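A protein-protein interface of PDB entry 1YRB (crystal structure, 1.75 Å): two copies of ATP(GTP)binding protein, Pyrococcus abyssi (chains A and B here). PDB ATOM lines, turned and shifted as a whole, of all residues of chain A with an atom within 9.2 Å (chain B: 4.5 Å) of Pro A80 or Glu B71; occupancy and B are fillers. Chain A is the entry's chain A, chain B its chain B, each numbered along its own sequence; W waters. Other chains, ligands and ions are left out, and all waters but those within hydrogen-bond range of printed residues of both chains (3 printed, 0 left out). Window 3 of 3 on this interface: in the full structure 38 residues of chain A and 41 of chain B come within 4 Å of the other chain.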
ATOM      1  N   THR A  51      23.239  16.885 -16.403  1.00  0.00           N
ATOM      2  CA  THR A  51      22.150  16.236 -17.127  1.00  0.00           C
ATOM      3  C   THR A  51      20.840  17.032 -17.099  1.00  0.00           C
ATOM      4  O   THR A  51      19.875  16.670 -17.793  1.00  0.00           O
ATOM      5  CB  THR A  51      21.871  14.832 -16.515  1.00  0.00           C
ATOM      6  OG1 THR A  51      21.670  14.978 -15.094  1.00  0.00           O
ATOM      7  CG2 THR A  51      23.042  13.895 -16.760  1.00  0.00           C
ATOM      8  N   GLY A  52      20.782  18.100 -16.298  1.00  0.00           N
ATOM      9  CA  GLY A  52      19.498  18.815 -16.096  1.00  0.00           C
ATOM     10  C   GLY A  52      19.216  20.033 -16.965  1.00  0.00           C
ATOM     11  O   GLY A  52      18.061  20.314 -17.344  1.00  0.00           O
ATOM     12  N   THR A  69      19.005  12.933 -20.229  1.00  0.00           N
ATOM     13  CA  THR A  69      18.650  14.136 -19.504  1.00  0.00           C
ATOM     14  C   THR A  69      17.754  13.796 -18.336  1.00  0.00           C
ATOM     15  O   THR A  69      17.066  12.770 -18.325  1.00  0.00           O
ATOM     16  CB  THR A  69      17.929  15.153 -20.408  1.00  0.00           C
ATOM     17  OG1 THR A  69      16.647  14.639 -20.801  1.00  0.00           O
ATOM     18  CG2 THR A  69      18.760  15.453 -21.649  1.00  0.00           C
ATOM     19  N   VAL A  70      17.741  14.688 -17.355  1.00  0.00           N
ATOM     20  CA  VAL A  70      16.853  14.532 -16.222  1.00  0.00           C
ATOM     21  C   VAL A  70      15.411  14.509 -16.714  1.00  0.00           C
ATOM     22  O   VAL A  70      14.601  13.716 -16.258  1.00  0.00           O
ATOM     23  CB  VAL A  70      17.053  15.709 -15.265  1.00  0.00           C
ATOM     24  CG1 VAL A  70      15.961  15.743 -14.192  1.00  0.00           C
ATOM     25  CG2 VAL A  70      18.425  15.593 -14.656  1.00  0.00           C
ATOM     26  N   GLU A  71      15.116  15.382 -17.670  1.00  0.00           N
ATOM     27  CA  GLU A  71      13.773  15.513 -18.216  1.00  0.00           C
ATOM     28  C   GLU A  71      13.316  14.213 -18.879  1.00  0.00           C
ATOM     29  O   GLU A  71      12.159  13.789 -18.711  1.00  0.00           O
ATOM     30  CB  GLU A  71      13.750  16.702 -19.182  1.00  0.00           C
ATOM     31  CG  GLU A  71      14.006  18.074 -18.478  1.00  0.00           C
ATOM     32  CD  GLU A  71      15.493  18.493 -18.291  1.00  0.00           C
ATOM     33  OE1 GLU A  71      16.462  17.694 -18.417  1.00  0.00           O
ATOM     34  OE2 GLU A  71      15.687  19.689 -17.998  1.00  0.00           O
ATOM     35  N   ILE A  73      14.297  11.190 -18.099  1.00  0.00           N
ATOM     36  CA  ILE A  73      14.069  10.244 -17.028  1.00  0.00           C
ATOM     37  C   ILE A  73      12.761  10.531 -16.293  1.00  0.00           C
ATOM     38  O   ILE A  73      12.050   9.612 -15.891  1.00  0.00           O
ATOM     39  CB  ILE A  73      15.294  10.205 -16.100  1.00  0.00           C
ATOM     40  CG1 ILE A  73      16.485   9.686 -16.911  1.00  0.00           C
ATOM     41  CG2 ILE A  73      15.066   9.315 -14.900  1.00  0.00           C
ATOM     42  CD1 ILE A  73      17.830   9.887 -16.242  1.00  0.00           C
ATOM     43  N   MET A  74      12.422  11.802 -16.156  1.00  0.00           N
ATOM     44  CA  MET A  74      11.172  12.168 -15.506  1.00  0.00           C
ATOM     45  C   MET A  74       9.982  11.689 -16.332  1.00  0.00           C
ATOM     46  O   MET A  74       8.946  11.319 -15.789  1.00  0.00           O
ATOM     47  CB  MET A  74      11.105  13.677 -15.292  1.00  0.00           C
ATOM     48  CG  MET A  74      12.010  14.126 -14.174  1.00  0.00           C
ATOM     49  SD  MET A  74      11.980  15.894 -13.901  1.00  0.00           S
ATOM     50  CE  MET A  74      10.398  16.036 -13.058  1.00  0.00           C
ATOM     51  N   ARG A  75      10.139  11.689 -17.647  1.00  0.00           N
ATOM     52  CA  ARG A  75       9.082  11.187 -18.518  1.00  0.00           C
ATOM     53  C   ARG A  75       8.821   9.711 -18.238  1.00  0.00           C
ATOM     54  O   ARG A  75       7.745   9.193 -18.563  1.00  0.00           O
ATOM     55  CB  ARG A  75       9.449  11.421 -19.988  1.00  0.00           C
ATOM     56  CG  ARG A  75       8.861  12.680 -20.628  1.00  0.00           C
ATOM     57  CD  ARG A  75       9.485  13.971 -20.107  1.00  0.00           C
ATOM     58  NE  ARG A  75       8.905  14.378 -18.832  1.00  0.00           N
ATOM     59  CZ  ARG A  75       9.364  15.371 -18.080  1.00  0.00           C
ATOM     60  NH1 ARG A  75      10.417  16.069 -18.470  1.00  0.00           N
ATOM     61  NH2 ARG A  75       8.765  15.667 -16.934  1.00  0.00           N
ATOM     62  N   GLY A  77       8.606   8.487 -15.248  1.00  0.00           N
ATOM     63  CA  GLY A  77       7.868   8.358 -13.998  1.00  0.00           C
ATOM     64  C   GLY A  77       8.609   8.848 -12.763  1.00  0.00           C
ATOM     65  O   GLY A  77       8.040   8.914 -11.666  1.00  0.00           O
ATOM     66  N   TYR A  78       9.880   9.190 -12.928  1.00  0.00           N
ATOM     67  CA  TYR A  78      10.686   9.659 -11.803  1.00  0.00           C
ATOM     68  C   TYR A  78      10.341  11.094 -11.458  1.00  0.00           C
ATOM     69  O   TYR A  78      10.022  11.887 -12.339  1.00  0.00           O
ATOM     70  CB  TYR A  78      12.170   9.613 -12.150  1.00  0.00           C
ATOM     71  CG  TYR A  78      12.776   8.242 -12.226  1.00  0.00           C
ATOM     72  CD1 TYR A  78      13.487   7.726 -11.155  1.00  0.00           C
ATOM     73  CD2 TYR A  78      12.669   7.475 -13.383  1.00  0.00           C
ATOM     74  CE1 TYR A  78      14.064   6.485 -11.223  1.00  0.00           C
ATOM     75  CE2 TYR A  78      13.254   6.230 -13.461  1.00  0.00           C
ATOM     76  CZ  TYR A  78      13.936   5.740 -12.372  1.00  0.00           C
ATOM     77  OH  TYR A  78      14.530   4.502 -12.428  1.00  0.00           O
ATOM     78  N   GLY A  79      10.421  11.431 -10.174  1.00  0.00           N
ATOM     79  CA  GLY A  79      10.334  12.822  -9.763  1.00  0.00           C
ATOM     80  C   GLY A  79      11.684  13.458 -10.027  1.00  0.00           C
ATOM     81  O   GLY A  79      12.626  12.764 -10.398  1.00  0.00           O
ATOM     82  N   PRO A  80      11.796  14.777  -9.821  1.00  0.00           N
ATOM     83  CA  PRO A  80      13.016  15.459 -10.254  1.00  0.00           C
ATOM     84  C   PRO A  80      14.266  15.022  -9.514  1.00  0.00           C
ATOM     85  O   PRO A  80      15.307  14.816 -10.132  1.00  0.00           O
ATOM     86  CB  PRO A  80      12.714  16.943  -9.978  1.00  0.00           C
ATOM     87  CG  PRO A  80      11.697  16.921  -8.867  1.00  0.00           C
ATOM     88  CD  PRO A  80      10.841  15.698  -9.181  1.00  0.00           C
ATOM     89  N   ASN A  81      14.212  14.908  -8.191  1.00  0.00           N
ATOM     90  CA  ASN A  81      15.407  14.483  -7.471  1.00  0.00           C
ATOM     91  C   ASN A  81      15.770  13.015  -7.690  1.00  0.00           C
ATOM     92  O   ASN A  81      16.951  12.670  -7.770  1.00  0.00           O
ATOM     93  CB  ASN A  81      15.316  14.852  -5.981  1.00  0.00           C
ATOM     94  CG  ASN A  81      15.378  16.341  -5.774  1.00  0.00           C
ATOM     95  OD1 ASN A  81      16.306  16.991  -6.247  1.00  0.00           O
ATOM     96  ND2 ASN A  81      14.375  16.902  -5.110  1.00  0.00           N
ATOM     97  N   GLY A  82      14.752  12.159  -7.804  1.00  0.00           N
ATOM     98  CA  GLY A  82      14.972  10.764  -8.160  1.00  0.00           C
ATOM     99  C   GLY A  82      15.618  10.684  -9.539  1.00  0.00           C
ATOM    100  O   GLY A  82      16.509   9.879  -9.766  1.00  0.00           O
ATOM    101  N   ALA A  83      15.178  11.545 -10.438  1.00  0.00           N
ATOM    102  CA  ALA A  83      15.686  11.583 -11.816  1.00  0.00           C
ATOM    103  C   ALA A  83      17.103  12.085 -11.887  1.00  0.00           C
ATOM    104  O   ALA A  83      17.906  11.616 -12.692  1.00  0.00           O
ATOM    105  CB  ALA A  83      14.777  12.445 -12.703  1.00  0.00           C
ATOM    106  N   ILE A  84      17.434  13.085 -11.072  1.00  0.00           N
ATOM    107  CA  ILE A  84      18.813  13.539 -11.065  1.00  0.00           C
ATOM    108  C   ILE A  84      19.754  12.404 -10.682  1.00  0.00           C
ATOM    109  O   ILE A  84      20.727  12.116 -11.398  1.00  0.00           O
ATOM    110  CB  ILE A  84      18.983  14.734 -10.118  1.00  0.00           C
ATOM    111  CG1 ILE A  84      18.214  15.925 -10.681  1.00  0.00           C
ATOM    112  CG2 ILE A  84      20.429  15.020  -9.922  1.00  0.00           C
ATOM    113  CD1 ILE A  84      17.921  17.048  -9.650  1.00  0.00           C
ATOM    114  N   VAL A  85      19.462  11.727  -9.577  1.00  0.00           N
ATOM    115  CA  VAL A  85      20.311  10.620  -9.161  1.00  0.00           C
ATOM    116  C   VAL A  85      20.326   9.494 -10.208  1.00  0.00           C
ATOM    117  O   VAL A  85      21.378   8.970 -10.550  1.00  0.00           O
ATOM    118  CB  VAL A  85      19.922  10.088  -7.785  1.00  0.00           C
ATOM    119  CG1 VAL A  85      20.820   8.906  -7.417  1.00  0.00           C
ATOM    120  CG2 VAL A  85      20.072  11.196  -6.762  1.00  0.00           C
ATOM    121  N   GLU A  86      19.163   9.135 -10.714  1.00  0.00           N
ATOM    122  CA  GLU A  86      19.112   8.081 -11.745  1.00  0.00           C
ATOM    123  C   GLU A  86      19.987   8.462 -12.957  1.00  0.00           C
ATOM    124  O   GLU A  86      20.711   7.625 -13.508  1.00  0.00           O
ATOM    125  CB  GLU A  86      17.668   7.815 -12.145  1.00  0.00           C
ATOM    126  CG  GLU A  86      17.472   6.746 -13.234  1.00  0.00           C
ATOM    127  CD  GLU A  86      17.931   5.357 -12.815  1.00  0.00           C
ATOM    128  OE1 GLU A  86      18.132   4.486 -13.699  1.00  0.00           O
ATOM    129  OE2 GLU A  86      18.102   5.116 -11.603  1.00  0.00           O
ATOM    130  N   SER A  87      19.960   9.734 -13.354  1.00  0.00           N
ATOM    131  CA  SER A  87      20.765  10.159 -14.510  1.00  0.00           C
ATOM    132  C   SER A  87      22.255   9.839 -14.327  1.00  0.00           C
ATOM    133  O   SER A  87      22.929   9.379 -15.257  1.00  0.00           O
ATOM    134  CB  SER A  87      20.524  11.645 -14.865  1.00  0.00           C
ATOM    135  OG  SER A  87      21.267  12.519 -14.010  1.00  0.00           O
ATOM    136  N   TYR A  88      22.782  10.040 -13.123  1.00  0.00           N
ATOM    137  CA  TYR A  88      24.196   9.782 -12.913  1.00  0.00           C
ATOM    138  C   TYR A  88      24.504   8.299 -12.748  1.00  0.00           C
ATOM    139  O   TYR A  88      25.608   7.860 -13.073  1.00  0.00           O
ATOM    140  CB  TYR A  88      24.784  10.657 -11.789  1.00  0.00           C
ATOM    141  CG  TYR A  88      24.825  12.067 -12.325  1.00  0.00           C
ATOM    142  CD1 TYR A  88      25.836  12.464 -13.193  1.00  0.00           C
ATOM    143  CD2 TYR A  88      23.781  12.942 -12.093  1.00  0.00           C
ATOM    144  CE1 TYR A  88      25.847  13.735 -13.761  1.00  0.00           C
ATOM    145  CE2 TYR A  88      23.773  14.212 -12.655  1.00  0.00           C
ATOM    146  CZ  TYR A  88      24.808  14.598 -13.489  1.00  0.00           C
ATOM    147  OH  TYR A  88      24.804  15.844 -14.061  1.00  0.00           O
ATOM    148  N   GLN A 119      23.585  20.208  -9.086  1.00  0.00           N
ATOM    149  CA  GLN A 119      23.644  19.970  -7.653  1.00  0.00           C
ATOM    150  C   GLN A 119      25.042  19.508  -7.291  1.00  0.00           C
ATOM    151  O   GLN A 119      25.474  18.439  -7.689  1.00  0.00           O
ATOM    152  CB  GLN A 119      22.624  18.919  -7.220  1.00  0.00           C
ATOM    153  CG  GLN A 119      21.181  19.261  -7.576  1.00  0.00           C
ATOM    154  CD  GLN A 119      20.614  20.404  -6.761  1.00  0.00           C
ATOM    155  OE1 GLN A 119      21.131  20.748  -5.690  1.00  0.00           O
ATOM    156  NE2 GLN A 119      19.527  20.995  -7.257  1.00  0.00           N
ATOM    157  N   THR A 122      25.654  15.966  -6.167  1.00  0.00           N
ATOM    158  CA  THR A 122      25.704  14.911  -7.160  1.00  0.00           C
ATOM    159  C   THR A 122      27.173  14.673  -7.480  1.00  0.00           C
ATOM    160  O   THR A 122      27.602  13.534  -7.665  1.00  0.00           O
ATOM    161  CB  THR A 122      24.917  15.263  -8.454  1.00  0.00           C
ATOM    162  OG1 THR A 122      23.597  15.723  -8.117  1.00  0.00           O
ATOM    163  CG2 THR A 122      24.794  14.024  -9.321  1.00  0.00           C
ATOM    164  N   THR B  51       9.821  20.070  -2.033  1.00  0.00           N
ATOM    165  CA  THR B  51       8.923  20.513  -3.112  1.00  0.00           C
ATOM    166  C   THR B  51       8.949  19.555  -4.310  1.00  0.00           C
ATOM    167  O   THR B  51       8.155  19.678  -5.244  1.00  0.00           O
ATOM    168  CB  THR B  51       9.337  21.913  -3.607  1.00  0.00           C
ATOM    169  OG1 THR B  51      10.742  21.918  -3.872  1.00  0.00           O
ATOM    170  CG2 THR B  51       9.065  22.963  -2.530  1.00  0.00           C
ATOM    171  N   GLY B  52       9.876  18.606  -4.292  1.00  0.00           N
ATOM    172  CA  GLY B  52      10.109  17.756  -5.468  1.00  0.00           C
ATOM    173  C   GLY B  52       9.353  16.445  -5.493  1.00  0.00           C
ATOM    174  O   GLY B  52       8.899  15.993  -6.547  1.00  0.00           O
ATOM    175  N   VAL B  53       9.189  15.825  -4.337  1.00  0.00           N
ATOM    176  CA  VAL B  53       8.778  14.430  -4.290  1.00  0.00           C
ATOM    177  C   VAL B  53       7.356  14.252  -4.819  1.00  0.00           C
ATOM    178  O   VAL B  53       6.517  15.136  -4.652  1.00  0.00           O
ATOM    179  CB  VAL B  53       8.915  13.890  -2.859  1.00  0.00           C
ATOM    180  CG1 VAL B  53       8.048  14.705  -1.911  1.00  0.00           C
ATOM    181  CG2 VAL B  53       8.593  12.397  -2.791  1.00  0.00           C
ATOM    182  N   LYS B  54       7.117  13.126  -5.494  1.00  0.00           N
ATOM    183  CA  LYS B  54       5.787  12.806  -6.050  1.00  0.00           C
ATOM    184  C   LYS B  54       4.838  12.172  -5.032  1.00  0.00           C
ATOM    185  O   LYS B  54       3.687  12.591  -4.916  1.00  0.00           O
ATOM    186  CB  LYS B  54       5.921  11.886  -7.281  1.00  0.00           C
ATOM    187  CG  LYS B  54       6.536  12.566  -8.499  1.00  0.00           C
ATOM    188  CD  LYS B  54       6.754  11.594  -9.655  1.00  0.00           C
ATOM    189  CE  LYS B  54       5.455  11.286 -10.394  1.00  0.00           C
ATOM    190  NZ  LYS B  54       5.713  10.809 -11.797  1.00  0.00           N
ATOM    191  N   THR B  69       5.246  23.004  -6.343  1.00  0.00           N
ATOM    192  CA  THR B  69       6.054  21.826  -6.597  1.00  0.00           C
ATOM    193  C   THR B  69       7.090  22.128  -7.676  1.00  0.00           C
ATOM    194  O   THR B  69       6.920  23.040  -8.488  1.00  0.00           O
ATOM    195  CB  THR B  69       5.215  20.629  -7.073  1.00  0.00           C
ATOM    196  OG1 THR B  69       4.604  20.941  -8.335  1.00  0.00           O
ATOM    197  CG2 THR B  69       4.125  20.283  -6.071  1.00  0.00           C
ATOM    198  N   VAL B  70       8.157  21.335  -7.693  1.00  0.00           N
ATOM    199  CA  VAL B  70       9.200  21.517  -8.679  1.00  0.00           C
ATOM    200  C   VAL B  70       8.601  21.242 -10.052  1.00  0.00           C
ATOM    201  O   VAL B  70       8.851  21.982 -10.998  1.00  0.00           O
ATOM    202  CB  VAL B  70      10.392  20.564  -8.426  1.00  0.00           C
ATOM    203  CG1 VAL B  70      11.403  20.645  -9.564  1.00  0.00           C
ATOM    204  CG2 VAL B  70      11.071  20.905  -7.108  1.00  0.00           C
ATOM    205  N   GLU B  71       7.801  20.187 -10.142  1.00  0.00           N
ATOM    206  CA  GLU B  71       7.173  19.798 -11.412  1.00  0.00           C
ATOM    207  C   GLU B  71       6.314  20.932 -12.021  1.00  0.00           C
ATOM    208  O   GLU B  71       6.411  21.232 -13.234  1.00  0.00           O
ATOM    209  CB  GLU B  71       6.414  18.474 -11.223  1.00  0.00           C
ATOM    210  CG  GLU B  71       7.326  17.299 -10.765  1.00  0.00           C
ATOM    211  CD  GLU B  71       7.516  17.135  -9.232  1.00  0.00           C
ATOM    212  OE1 GLU B  71       7.462  18.112  -8.438  1.00  0.00           O
ATOM    213  OE2 GLU B  71       7.753  15.975  -8.816  1.00  0.00           O
ATOM    214  N   GLU B  72       5.522  21.594 -11.185  1.00  0.00           N
ATOM    215  CA  GLU B  72       4.809  22.807 -11.624  1.00  0.00           C
ATOM    216  C   GLU B  72       5.731  23.908 -12.154  1.00  0.00           C
ATOM    217  O   GLU B  72       5.459  24.519 -13.194  1.00  0.00           O
ATOM    218  CB  GLU B  72       3.939  23.381 -10.501  1.00  0.00           C
ATOM    219  CG  GLU B  72       3.322  24.732 -10.836  1.00  0.00           C
ATOM    220  CD  GLU B  72       2.023  24.606 -11.598  1.00  0.00           C
ATOM    221  OE1 GLU B  72       1.449  25.651 -11.971  1.00  0.00           O
ATOM    222  OE2 GLU B  72       1.574  23.466 -11.818  1.00  0.00           O
ATOM    223  N   ILE B  73       6.815  24.180 -11.446  1.00  0.00           N
ATOM    224  CA  ILE B  73       7.733  25.228 -11.871  1.00  0.00           C
ATOM    225  C   ILE B  73       8.415  24.858 -13.197  1.00  0.00           C
ATOM    226  O   ILE B  73       8.694  25.731 -14.030  1.00  0.00           O
ATOM    227  CB  ILE B  73       8.748  25.564 -10.762  1.00  0.00           C
ATOM    228  CG1 ILE B  73       8.013  26.172  -9.558  1.00  0.00           C
ATOM    229  CG2 ILE B  73       9.786  26.548 -11.247  1.00  0.00           C
ATOM    230  CD1 ILE B  73       8.932  26.487  -8.395  1.00  0.00           C
ATOM    231  N   MET B  74       8.657  23.566 -13.411  1.00  0.00           N
ATOM    232  CA  MET B  74       9.296  23.130 -14.658  1.00  0.00           C
ATOM    233  C   MET B  74       8.323  23.298 -15.831  1.00  0.00           C
ATOM    234  O   MET B  74       8.738  23.509 -16.971  1.00  0.00           O
ATOM    235  CB  MET B  74       9.757  21.675 -14.552  1.00  0.00           C
ATOM    236  CG  MET B  74      10.976  21.466 -13.633  1.00  0.00           C
ATOM    237  SD  MET B  74      11.416  19.728 -13.499  1.00  0.00           S
ATOM    238  CE  MET B  74      11.829  19.345 -15.218  1.00  0.00           C
ATOM    239  N   ARG B  75       7.029  23.200 -15.551  1.00  0.00           N
ATOM    240  CA  ARG B  75       6.009  23.426 -16.584  1.00  0.00           C
ATOM    241  C   ARG B  75       6.046  24.864 -17.104  1.00  0.00           C
ATOM    242  O   ARG B  75       5.587  25.130 -18.224  1.00  0.00           O
ATOM    243  CB  ARG B  75       4.608  23.124 -16.039  1.00  0.00           C
ATOM    244  CG  ARG B  75       4.245  21.640 -15.993  1.00  0.00           C
ATOM    245  CD  ARG B  75       3.018  21.384 -15.118  1.00  0.00           C
ATOM    246  NE  ARG B  75       1.773  21.402 -15.878  1.00  0.00           N
ATOM    247  CZ  ARG B  75       0.971  22.455 -15.975  1.00  0.00           C
ATOM    248  NH1 ARG B  75       1.281  23.586 -15.358  1.00  0.00           N
ATOM    249  NH2 ARG B  75      -0.143  22.378 -16.690  1.00  0.00           N
HETATM  250  O   HOH W   1       7.747  12.806 -13.230  1.00  0.00           O
HETATM  251  O   HOH W   2       5.358   8.232 -11.379  1.00  0.00           O
HETATM  252  O   HOH W   3      13.126  19.855  -4.026  1.00  0.00           O
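Met B74 touches its own counterpart, Met A74. 8 positions are printed for both chains. Of the 6 pairs that touch across the chains among the printed residues, 1 has its exchanged pair printed and touching as well.
Printed residues of chain B that touch a printed residue of chain A: Gly B52, Lys B54, Val B70, Glu B71 and Met B74. Hydrophobic or aromatic side chains of chain B within 4 Å of the printed part of chain A: Val B70 and Met B74. Among the printed residues, 6 pairs touch across the chains.
Water W1 lies within hydrogen-bond range of O of Tyr A78 (2.6 Å), NZ of Lys B54 (3.2 Å) and O of Met A74 (3.2 Å). Water W2 lies within hydrogen-bond range of NZ of Lys B54 (2.6 Å) and O of Gly A77 (2.8 Å). Water W3 lies within hydrogen-bond range of the side-chain hydroxyl (OG1) of Thr B51 (3.2 Å), the side-chain amide nitrogen (ND2) of Asn A81 (3.4 Å) and the backbone NH (N) of Gly B52 (3.5 Å).
Of the printed residues of chain B, Pro A80 touches Gly B52, Val B70 and Glu B71. Printed residues of chain A within 4 Å of Glu B71: Pro A80 (3.1 Å). Printed residues of chain A within 4 Å of Met B74: Met A74. Printed residues of chain B within 4 Å of Gly A77: Lys B54. Of the printed residues of chain A, Lys B54 touches Gly A77 (3.0 Å) and Gly A79 (3.7 Å). Ile A73 touches none of the printed residues of chain B. The nearest printed residue of chain B that does not touch Met A74 is Glu B71 (4.04 Å).
O of Gly A77 is in hydrogen-bond range of NZ of Lys B54, at 3.0 Å.
The backbone carbonyl oxygen of Thr B51 is in hydrogen-bond range of the backbone NH of Val B70 (3.0 Å). The backbone carbonyl oxygen (O) of Gly B52 lies close to the side-chain carboxylate (OE2) of Glu B71 (2.5 Å).
Among the printed residues, pairs that only touch across the chains: Met A74 with Met B74 (3.7 Å), Gly A79 with Lys B54 (3.7 Å), Pro A80 with Gly B52 (3.3 Å), Pro A80 with Val B70 (3.8 Å) and Pro A80 with Glu B71 (3.1 Å).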
